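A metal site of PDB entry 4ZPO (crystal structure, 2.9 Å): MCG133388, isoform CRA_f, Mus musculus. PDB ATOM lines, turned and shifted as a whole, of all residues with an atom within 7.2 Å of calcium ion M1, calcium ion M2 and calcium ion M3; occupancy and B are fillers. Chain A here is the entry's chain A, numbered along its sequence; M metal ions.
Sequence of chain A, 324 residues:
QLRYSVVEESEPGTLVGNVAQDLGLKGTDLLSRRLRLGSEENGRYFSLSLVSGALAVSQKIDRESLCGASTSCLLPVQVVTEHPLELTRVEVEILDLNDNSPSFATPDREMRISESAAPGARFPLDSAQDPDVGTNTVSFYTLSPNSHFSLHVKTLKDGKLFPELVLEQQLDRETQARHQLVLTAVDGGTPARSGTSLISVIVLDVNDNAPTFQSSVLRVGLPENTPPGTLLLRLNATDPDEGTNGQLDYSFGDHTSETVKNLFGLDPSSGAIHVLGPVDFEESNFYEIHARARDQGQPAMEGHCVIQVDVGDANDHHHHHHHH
Within 4 Å of calcium ion M3: Asn 98, Asn 100, Asp 130, Asp 132, Asn 136 and Asp 187.
Along chain A the residues within 4 Å of calcium ion M3 span positions 98 to 187.
N of Glu 8 is in hydrogen-bond range of O of Leu 95, 3.2 Å away.
The side-chain carboxylate (OE2) of Glu 8 sits close to the backbone NH (N) of Arg 63 (3.3 Å).
OG of Ser 65 is in hydrogen-bond range of OD2 of Asp 62 (2.6 Å).
OD1 of Asp 187 lies within hydrogen-bond range of N of Gly 189 (3.2 Å).
OD2 of Asp 96 lies within hydrogen-bond range of ND2 of Asn 136 (3.0 Å).
The backbone carbonyl oxygen (O) of Asn 98 is in hydrogen-bond range of the guanidinium group (NH1) of Arg 193, at 2.8 Å.
The backbone carbonyl oxygen of Asp 130 sits at hydrogen-bond distance from the side-chain hydroxyl of Thr 137, at 3.0 Å.
The side-chain carboxylate (OE2) of Glu 64 sits close to the side-chain amide nitrogen (ND2) of Asn 100 (3.1 Å).
Calcium ion M3 is bound by O of Asn 100 (2.4 Å), OD1 of Asn 98 (2.5 Å), O of Asn 136 (2.5 Å), OD2 of Asp 130 (2.6 Å), OD2 of Asp 132 (2.6 Å) and OD1 of Asp 130 (2.7 Å).
Slightly farther from calcium ion M3 lies OD2 of Asp 187 (3.0 Å).
The nearest printed residue that does not touch calcium ion M1 is Arg 63 (4.8 Å).
O of Leu 97 binds calcium ion M2, 2.4 Å away.
The side-chain carboxylate (OE2) of Glu 64 binds calcium ion M2, at 2.5 Å.
Calcium ion M2 is bound by OE1 of Glu 64, 2.6 Å away.
OD1 of Asp 132 is bound to calcium ion M2, at 2.6 Å.
The side-chain carboxylate (OD1) of Asp 96 binds calcium ion M2 (2.6 Å).
OE1 of Glu 8 binds calcium ion M2, 2.7 Å away.
OD1 of Asp 99 is bound to calcium ion M2, 2.8 Å away.
Calcium ion M2 has seven donor atoms within binding distance.
Along chain A the residues within 4 Å of calcium ion M2 span positions 8 to 132.
The nearest printed residue that does not touch calcium ion M2 is Arg 63 (4.3 Å).
OD1 of Asp 62 is bound to calcium ion M1, 2.4 Å away.
Calcium ion M1 is bound by the side-chain carboxylate (OE2) of Glu 8, at 2.4 Å.
Calcium ion M1 is bound by OD2 of Asp 99 (2.6 Å).
OE2 of Glu 64 binds calcium ion M1, 2.6 Å away.
Calcium ion M1 is bound by OE2 of Glu 9 (2.7 Å).
Calcium ion M1 has five donor atoms within binding distance.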
ATOM      1  N   GLU A   8     -23.987  11.714   4.793  1.00  0.00           N
ATOM      2  CA  GLU A   8     -25.378  11.257   4.782  1.00  0.00           C
ATOM      3  C   GLU A   8     -26.292  12.324   4.192  1.00  0.00           C
ATOM      4  O   GLU A   8     -26.000  13.521   4.280  1.00  0.00           O
ATOM      5  CB  GLU A   8     -25.812  10.906   6.209  1.00  0.00           C
ATOM      6  CG  GLU A   8     -27.229  10.380   6.339  1.00  0.00           C
ATOM      7  CD  GLU A   8     -27.800  10.614   7.722  1.00  0.00           C
ATOM      8  OE1 GLU A   8     -27.055  11.085   8.602  1.00  0.00           O
ATOM      9  OE2 GLU A   8     -29.007  10.349   7.922  1.00  0.00           O
ATOM     10  N   GLU A   9     -27.388  11.880   3.566  1.00  0.00           N
ATOM     11  CA  GLU A   9     -28.416  12.766   3.007  1.00  0.00           C
ATOM     12  C   GLU A   9     -27.897  13.641   1.863  1.00  0.00           C
ATOM     13  O   GLU A   9     -28.518  14.643   1.509  1.00  0.00           O
ATOM     14  CB  GLU A   9     -29.010  13.662   4.097  1.00  0.00           C
ATOM     15  CG  GLU A   9     -29.479  12.930   5.338  1.00  0.00           C
ATOM     16  CD  GLU A   9     -30.697  12.068   5.092  1.00  0.00           C
ATOM     17  OE1 GLU A   9     -31.370  12.254   4.051  1.00  0.00           O
ATOM     18  OE2 GLU A   9     -30.988  11.191   5.932  1.00  0.00           O
ATOM     19  N   ILE A  61     -28.992   8.568   0.708  1.00  0.00           N
ATOM     20  CA  ILE A  61     -28.671   7.586   1.733  1.00  0.00           C
ATOM     21  C   ILE A  61     -29.032   8.068   3.134  1.00  0.00           C
ATOM     22  O   ILE A  61     -28.616   9.150   3.553  1.00  0.00           O
ATOM     23  CB  ILE A  61     -27.177   7.208   1.715  1.00  0.00           C
ATOM     24  CG1 ILE A  61     -26.811   6.573   0.368  1.00  0.00           C
ATOM     25  CG2 ILE A  61     -26.834   6.273   2.861  1.00  0.00           C
ATOM     26  CD1 ILE A  61     -25.340   6.268   0.219  1.00  0.00           C
ATOM     27  N   ASP A  62     -29.790   7.254   3.865  1.00  0.00           N
ATOM     28  CA  ASP A  62     -30.128   7.558   5.255  1.00  0.00           C
ATOM     29  C   ASP A  62     -29.302   6.678   6.184  1.00  0.00           C
ATOM     30  O   ASP A  62     -29.490   5.467   6.235  1.00  0.00           O
ATOM     31  CB  ASP A  62     -31.630   7.342   5.502  1.00  0.00           C
ATOM     32  CG  ASP A  62     -32.056   7.812   6.878  1.00  0.00           C
ATOM     33  OD1 ASP A  62     -31.407   8.717   7.434  1.00  0.00           O
ATOM     34  OD2 ASP A  62     -33.043   7.262   7.405  1.00  0.00           O
ATOM     35  N   ARG A  63     -28.395   7.304   6.926  1.00  0.00           N
ATOM     36  CA  ARG A  63     -27.482   6.559   7.791  1.00  0.00           C
ATOM     37  C   ARG A  63     -28.214   5.859   8.931  1.00  0.00           C
ATOM     38  O   ARG A  63     -27.799   4.791   9.390  1.00  0.00           O
ATOM     39  CB  ARG A  63     -26.410   7.486   8.371  1.00  0.00           C
ATOM     40  CG  ARG A  63     -25.250   6.757   9.015  1.00  0.00           C
ATOM     41  CD  ARG A  63     -24.726   7.505  10.231  1.00  0.00           C
ATOM     42  NE  ARG A  63     -25.761   7.631  11.259  1.00  0.00           N
ATOM     43  CZ  ARG A  63     -25.977   6.723  12.208  1.00  0.00           C
ATOM     44  NH1 ARG A  63     -26.942   6.914  13.092  1.00  0.00           N
ATOM     45  NH2 ARG A  63     -25.233   5.623  12.259  1.00  0.00           N
ATOM     46  N   GLU A  64     -29.305   6.460   9.383  1.00  0.00           N
ATOM     47  CA  GLU A  64     -30.098   5.887  10.474  1.00  0.00           C
ATOM     48  C   GLU A  64     -30.819   4.615  10.049  1.00  0.00           C
ATOM     49  O   GLU A  64     -31.089   3.732  10.866  1.00  0.00           O
ATOM     50  CB  GLU A  64     -31.108   6.902  11.001  1.00  0.00           C
ATOM     51  CG  GLU A  64     -30.536   7.906  12.004  1.00  0.00           C
ATOM     52  CD  GLU A  64     -29.509   8.835  11.396  1.00  0.00           C
ATOM     53  OE1 GLU A  64     -28.349   8.822  11.842  1.00  0.00           O
ATOM     54  OE2 GLU A  64     -29.881   9.585  10.464  1.00  0.00           O
ATOM     55  N   SER A  65     -31.131   4.516   8.757  1.00  0.00           N
ATOM     56  CA  SER A  65     -31.857   3.375   8.228  1.00  0.00           C
ATOM     57  C   SER A  65     -30.951   2.180   7.960  1.00  0.00           C
ATOM     58  O   SER A  65     -31.392   1.028   7.986  1.00  0.00           O
ATOM     59  CB  SER A  65     -32.599   3.756   6.949  1.00  0.00           C
ATOM     60  OG  SER A  65     -33.592   4.739   7.211  1.00  0.00           O
ATOM     61  N   LEU A  95     -20.795   9.140   6.799  1.00  0.00           N
ATOM     62  CA  LEU A  95     -20.635  10.103   7.878  1.00  0.00           C
ATOM     63  C   LEU A  95     -21.988  10.555   8.422  1.00  0.00           C
ATOM     64  O   LEU A  95     -22.905  10.852   7.661  1.00  0.00           O
ATOM     65  CB  LEU A  95     -19.825  11.311   7.393  1.00  0.00           C
ATOM     66  CG  LEU A  95     -18.456  11.000   6.797  1.00  0.00           C
ATOM     67  CD1 LEU A  95     -17.751  12.279   6.372  1.00  0.00           C
ATOM     68  CD2 LEU A  95     -17.599  10.212   7.772  1.00  0.00           C
ATOM     69  N   ASP A  96     -22.100  10.603   9.742  1.00  0.00           N
ATOM     70  CA  ASP A  96     -23.362  10.941  10.390  1.00  0.00           C
ATOM     71  C   ASP A  96     -23.672  12.430  10.305  1.00  0.00           C
ATOM     72  O   ASP A  96     -22.806  13.282  10.511  1.00  0.00           O
ATOM     73  CB  ASP A  96     -23.342  10.512  11.858  1.00  0.00           C
ATOM     74  CG  ASP A  96     -24.611  10.890  12.593  1.00  0.00           C
ATOM     75  OD1 ASP A  96     -25.696  10.851  11.980  1.00  0.00           O
ATOM     76  OD2 ASP A  96     -24.532  11.239  13.796  1.00  0.00           O
ATOM     77  N   LEU A  97     -24.930  12.742  10.007  1.00  0.00           N
ATOM     78  CA  LEU A  97     -25.416  14.113   9.988  1.00  0.00           C
ATOM     79  C   LEU A  97     -26.381  14.317  11.150  1.00  0.00           C
ATOM     80  O   LEU A  97     -27.058  13.386  11.576  1.00  0.00           O
ATOM     81  CB  LEU A  97     -26.107  14.416   8.650  1.00  0.00           C
ATOM     82  CG  LEU A  97     -26.102  15.865   8.164  1.00  0.00           C
ATOM     83  CD1 LEU A  97     -24.685  16.342   7.912  1.00  0.00           C
ATOM     84  CD2 LEU A  97     -26.953  16.002   6.912  1.00  0.00           C
ATOM     85  N   ASN A  98     -26.440  15.543  11.671  1.00  0.00           N
ATOM     86  CA  ASN A  98     -27.329  15.827  12.800  1.00  0.00           C
ATOM     87  C   ASN A  98     -28.685  16.321  12.333  1.00  0.00           C
ATOM     88  O   ASN A  98     -29.053  17.477  12.567  1.00  0.00           O
ATOM     89  CB  ASN A  98     -26.682  16.860  13.727  1.00  0.00           C
ATOM     90  CG  ASN A  98     -27.428  17.006  15.045  1.00  0.00           C
ATOM     91  OD1 ASN A  98     -27.991  16.039  15.564  1.00  0.00           O
ATOM     92  ND2 ASN A  98     -27.442  18.215  15.590  1.00  0.00           N
ATOM     93  N   ASP A  99     -29.439  15.447  11.665  1.00  0.00           N
ATOM     94  CA  ASP A  99     -30.723  15.829  11.091  1.00  0.00           C
ATOM     95  C   ASP A  99     -31.898  15.207  11.835  1.00  0.00           C
ATOM     96  O   ASP A  99     -33.048  15.291  11.385  1.00  0.00           O
ATOM     97  CB  ASP A  99     -30.772  15.436   9.621  1.00  0.00           C
ATOM     98  CG  ASP A  99     -30.456  13.975   9.387  1.00  0.00           C
ATOM     99  OD1 ASP A  99     -29.635  13.405  10.144  1.00  0.00           O
ATOM    100  OD2 ASP A  99     -31.029  13.386   8.445  1.00  0.00           O
ATOM    101  N   ASN A 100     -31.623  14.585  12.982  1.00  0.00           N
ATOM    102  CA  ASN A 100     -32.683  14.016  13.808  1.00  0.00           C
ATOM    103  C   ASN A 100     -32.837  14.766  15.130  1.00  0.00           C
ATOM    104  O   ASN A 100     -31.848  15.154  15.757  1.00  0.00           O
ATOM    105  CB  ASN A 100     -32.413  12.533  14.087  1.00  0.00           C
ATOM    106  CG  ASN A 100     -32.814  11.647  12.928  1.00  0.00           C
ATOM    107  OD1 ASN A 100     -33.953  11.173  12.863  1.00  0.00           O
ATOM    108  ND2 ASN A 100     -31.885  11.409  12.006  1.00  0.00           N
ATOM    109  N   SER A 101     -34.078  14.975  15.540  1.00  0.00           N
ATOM    110  CA  SER A 101     -34.375  15.721  16.765  1.00  0.00           C
ATOM    111  C   SER A 101     -34.827  14.786  17.887  1.00  0.00           C
ATOM    112  O   SER A 101     -35.522  13.797  17.624  1.00  0.00           O
ATOM    113  CB  SER A 101     -35.441  16.781  16.504  1.00  0.00           C
ATOM    114  OG  SER A 101     -35.037  17.669  15.474  1.00  0.00           O
ATOM    115  N   PRO A 102     -34.418  15.085  19.135  1.00  0.00           N
ATOM    116  CA  PRO A 102     -34.784  14.313  20.319  1.00  0.00           C
ATOM    117  C   PRO A 102     -36.287  14.053  20.421  1.00  0.00           C
ATOM    118  O   PRO A 102     -37.091  14.976  20.299  1.00  0.00           O
ATOM    119  CB  PRO A 102     -34.312  15.202  21.465  1.00  0.00           C
ATOM    120  CG  PRO A 102     -33.132  15.908  20.903  1.00  0.00           C
ATOM    121  CD  PRO A 102     -33.468  16.164  19.453  1.00  0.00           C
ATOM    122  N   GLN A 129     -35.155  10.053  22.901  1.00  0.00           N
ATOM    123  CA  GLN A 129     -34.391   9.278  21.933  1.00  0.00           C
ATOM    124  C   GLN A 129     -33.866  10.156  20.802  1.00  0.00           C
ATOM    125  O   GLN A 129     -34.545  11.090  20.362  1.00  0.00           O
ATOM    126  CB  GLN A 129     -35.239   8.144  21.360  1.00  0.00           C
ATOM    127  CG  GLN A 129     -35.778   7.185  22.404  1.00  0.00           C
ATOM    128  CD  GLN A 129     -36.823   6.249  21.838  1.00  0.00           C
ATOM    129  OE1 GLN A 129     -37.092   6.261  20.638  1.00  0.00           O
ATOM    130  NE2 GLN A 129     -37.418   5.444  22.695  1.00  0.00           N
ATOM    131  N   ASP A 130     -32.667   9.841  20.323  1.00  0.00           N
ATOM    132  CA  ASP A 130     -32.069  10.540  19.192  1.00  0.00           C
ATOM    133  C   ASP A 130     -31.245   9.543  18.387  1.00  0.00           C
ATOM    134  O   ASP A 130     -30.125   9.214  18.753  1.00  0.00           O
ATOM    135  CB  ASP A 130     -31.196  11.704  19.679  1.00  0.00           C
ATOM    136  CG  ASP A 130     -30.898  12.716  18.582  1.00  0.00           C
ATOM    137  OD1 ASP A 130     -30.863  12.323  17.397  1.00  0.00           O
ATOM    138  OD2 ASP A 130     -30.699  13.903  18.912  1.00  0.00           O
ATOM    139  N   PRO A 131     -31.809   9.075  17.261  1.00  0.00           N
ATOM    140  CA  PRO A 131     -31.206   8.006  16.445  1.00  0.00           C
ATOM    141  C   PRO A 131     -29.858   8.381  15.830  1.00  0.00           C
ATOM    142  O   PRO A 131     -29.217   7.516  15.236  1.00  0.00           O
ATOM    143  CB  PRO A 131     -32.250   7.779  15.348  1.00  0.00           C
ATOM    144  CG  PRO A 131     -33.014   9.051  15.276  1.00  0.00           C
ATOM    145  CD  PRO A 131     -33.072   9.557  16.680  1.00  0.00           C
ATOM    146  N   ASP A 132     -29.433   9.627  15.985  1.00  0.00           N
ATOM    147  CA  ASP A 132     -28.112  10.036  15.507  1.00  0.00           C
ATOM    148  C   ASP A 132     -27.016   9.422  16.362  1.00  0.00           C
ATOM    149  O   ASP A 132     -27.294   8.852  17.421  1.00  0.00           O
ATOM    150  CB  ASP A 132     -28.000  11.564  15.474  1.00  0.00           C
ATOM    151  CG  ASP A 132     -28.846  12.192  14.388  1.00  0.00           C
ATOM    152  OD1 ASP A 132     -29.177  11.487  13.403  1.00  0.00           O
ATOM    153  OD2 ASP A 132     -29.172  13.398  14.493  1.00  0.00           O
ATOM    154  N   VAL A 133     -25.775   9.555  15.920  1.00  0.00           N
ATOM    155  CA  VAL A 133     -24.659   8.849  16.561  1.00  0.00           C
ATOM    156  C   VAL A 133     -23.511   9.781  16.915  1.00  0.00           C
ATOM    157  O   VAL A 133     -23.128  10.657  16.138  1.00  0.00           O
ATOM    158  CB  VAL A 133     -24.150   7.710  15.643  1.00  0.00           C
ATOM    159  CG1 VAL A 133     -22.699   7.338  15.952  1.00  0.00           C
ATOM    160  CG2 VAL A 133     -25.054   6.494  15.762  1.00  0.00           C
ATOM    161  N   THR A 135     -21.855  12.704  19.132  1.00  0.00           N
ATOM    162  CA  THR A 135     -22.283  13.872  19.887  1.00  0.00           C
ATOM    163  C   THR A 135     -23.646  14.343  19.412  1.00  0.00           C
ATOM    164  O   THR A 135     -24.331  15.098  20.094  1.00  0.00           O
ATOM    165  CB  THR A 135     -21.268  15.029  19.765  1.00  0.00           C
ATOM    166  OG1 THR A 135     -21.176  15.444  18.395  1.00  0.00           O
ATOM    167  CG2 THR A 135     -19.889  14.590  20.250  1.00  0.00           C
ATOM    168  N   ASN A 136     -24.056  13.865  18.232  1.00  0.00           N
ATOM    169  CA  ASN A 136     -25.306  14.289  17.628  1.00  0.00           C
ATOM    170  C   ASN A 136     -26.541  13.696  18.304  1.00  0.00           C
ATOM    171  O   ASN A 136     -27.673  14.078  17.987  1.00  0.00           O
ATOM    172  CB  ASN A 136     -25.314  13.930  16.134  1.00  0.00           C
ATOM    173  CG  ASN A 136     -24.266  14.682  15.344  1.00  0.00           C
ATOM    174  OD1 ASN A 136     -23.882  15.795  15.708  1.00  0.00           O
ATOM    175  ND2 ASN A 136     -23.787  14.083  14.262  1.00  0.00           N
ATOM    176  N   THR A 137     -26.329  12.767  19.223  1.00  0.00           N
ATOM    177  CA  THR A 137     -27.438  12.186  19.985  1.00  0.00           C
ATOM    178  C   THR A 137     -27.679  13.001  21.252  1.00  0.00           C
ATOM    179  O   THR A 137     -26.963  13.968  21.518  1.00  0.00           O
ATOM    180  CB  THR A 137     -27.163  10.714  20.354  1.00  0.00           C
ATOM    181  OG1 THR A 137     -28.330  10.154  20.973  1.00  0.00           O
ATOM    182  CG2 THR A 137     -25.990  10.613  21.312  1.00  0.00           C
ATOM    183  N   VAL A 138     -28.689  12.601  22.022  1.00  0.00           N
ATOM    184  CA  VAL A 138     -29.101  13.311  23.240  1.00  0.00           C
ATOM    185  C   VAL A 138     -27.920  13.633  24.160  1.00  0.00           C
ATOM    186  O   VAL A 138     -27.142  12.756  24.516  1.00  0.00           O
ATOM    187  CB  VAL A 138     -30.140  12.488  24.040  1.00  0.00           C
ATOM    188  CG1 VAL A 138     -30.454  13.166  25.366  1.00  0.00           C
ATOM    189  CG2 VAL A 138     -31.402  12.297  23.219  1.00  0.00           C
ATOM    190  N   ASP A 187     -29.668  17.608  22.078  1.00  0.00           N
ATOM    191  CA  ASP A 187     -28.511  16.857  21.614  1.00  0.00           C
ATOM    192  C   ASP A 187     -27.279  17.759  21.597  1.00  0.00           C
ATOM    193  O   ASP A 187     -27.354  18.928  21.958  1.00  0.00           O
ATOM    194  CB  ASP A 187     -28.760  16.248  20.225  1.00  0.00           C
ATOM    195  CG  ASP A 187     -29.136  17.288  19.172  1.00  0.00           C
ATOM    196  OD1 ASP A 187     -28.410  18.303  19.027  1.00  0.00           O
ATOM    197  OD2 ASP A 187     -30.147  17.081  18.477  1.00  0.00           O
ATOM    198  N   GLY A 188     -26.138  17.204  21.177  1.00  0.00           N
ATOM    199  CA  GLY A 188     -24.894  17.944  21.174  1.00  0.00           C
ATOM    200  C   GLY A 188     -24.385  18.257  19.778  1.00  0.00           C
ATOM    201  O   GLY A 188     -23.211  18.036  19.477  1.00  0.00           O
ATOM    202  N   GLY A 189     -25.260  18.756  18.926  1.00  0.00           N
ATOM    203  CA  GLY A 189     -24.882  19.149  17.576  1.00  0.00           C
ATOM    204  C   GLY A 189     -24.790  20.654  17.439  1.00  0.00           C
ATOM    205  O   GLY A 189     -25.165  21.391  18.341  1.00  0.00           O
ATOM    206  N   ARG A 193     -30.434  20.516  18.448  1.00  0.00           N
ATOM    207  CA  ARG A 193     -31.849  20.280  18.189  1.00  0.00           C
ATOM    208  C   ARG A 193     -32.507  19.718  19.449  1.00  0.00           C
ATOM    209  O   ARG A 193     -31.861  19.008  20.221  1.00  0.00           O
ATOM    210  CB  ARG A 193     -32.035  19.318  17.020  1.00  0.00           C
ATOM    211  CG  ARG A 193     -31.012  19.534  15.910  1.00  0.00           C
ATOM    212  CD  ARG A 193     -31.160  18.494  14.812  1.00  0.00           C
ATOM    213  NE  ARG A 193     -32.221  18.830  13.875  1.00  0.00           N
ATOM    214  CZ  ARG A 193     -32.011  19.415  12.693  1.00  0.00           C
ATOM    215  NH1 ARG A 193     -30.788  19.706  12.303  1.00  0.00           N
ATOM    216  NH2 ARG A 193     -33.043  19.680  11.900  1.00  0.00           N
HETATM  217 CA    CA M   1     -31.268  10.809   8.626  1.00  0.00          CA
HETATM  218 CA    CA M   2     -28.103  11.255  11.050  1.00  0.00          CA
HETATM  219 CA    CA M   3     -29.690  14.662  16.689  1.00  0.00          CA
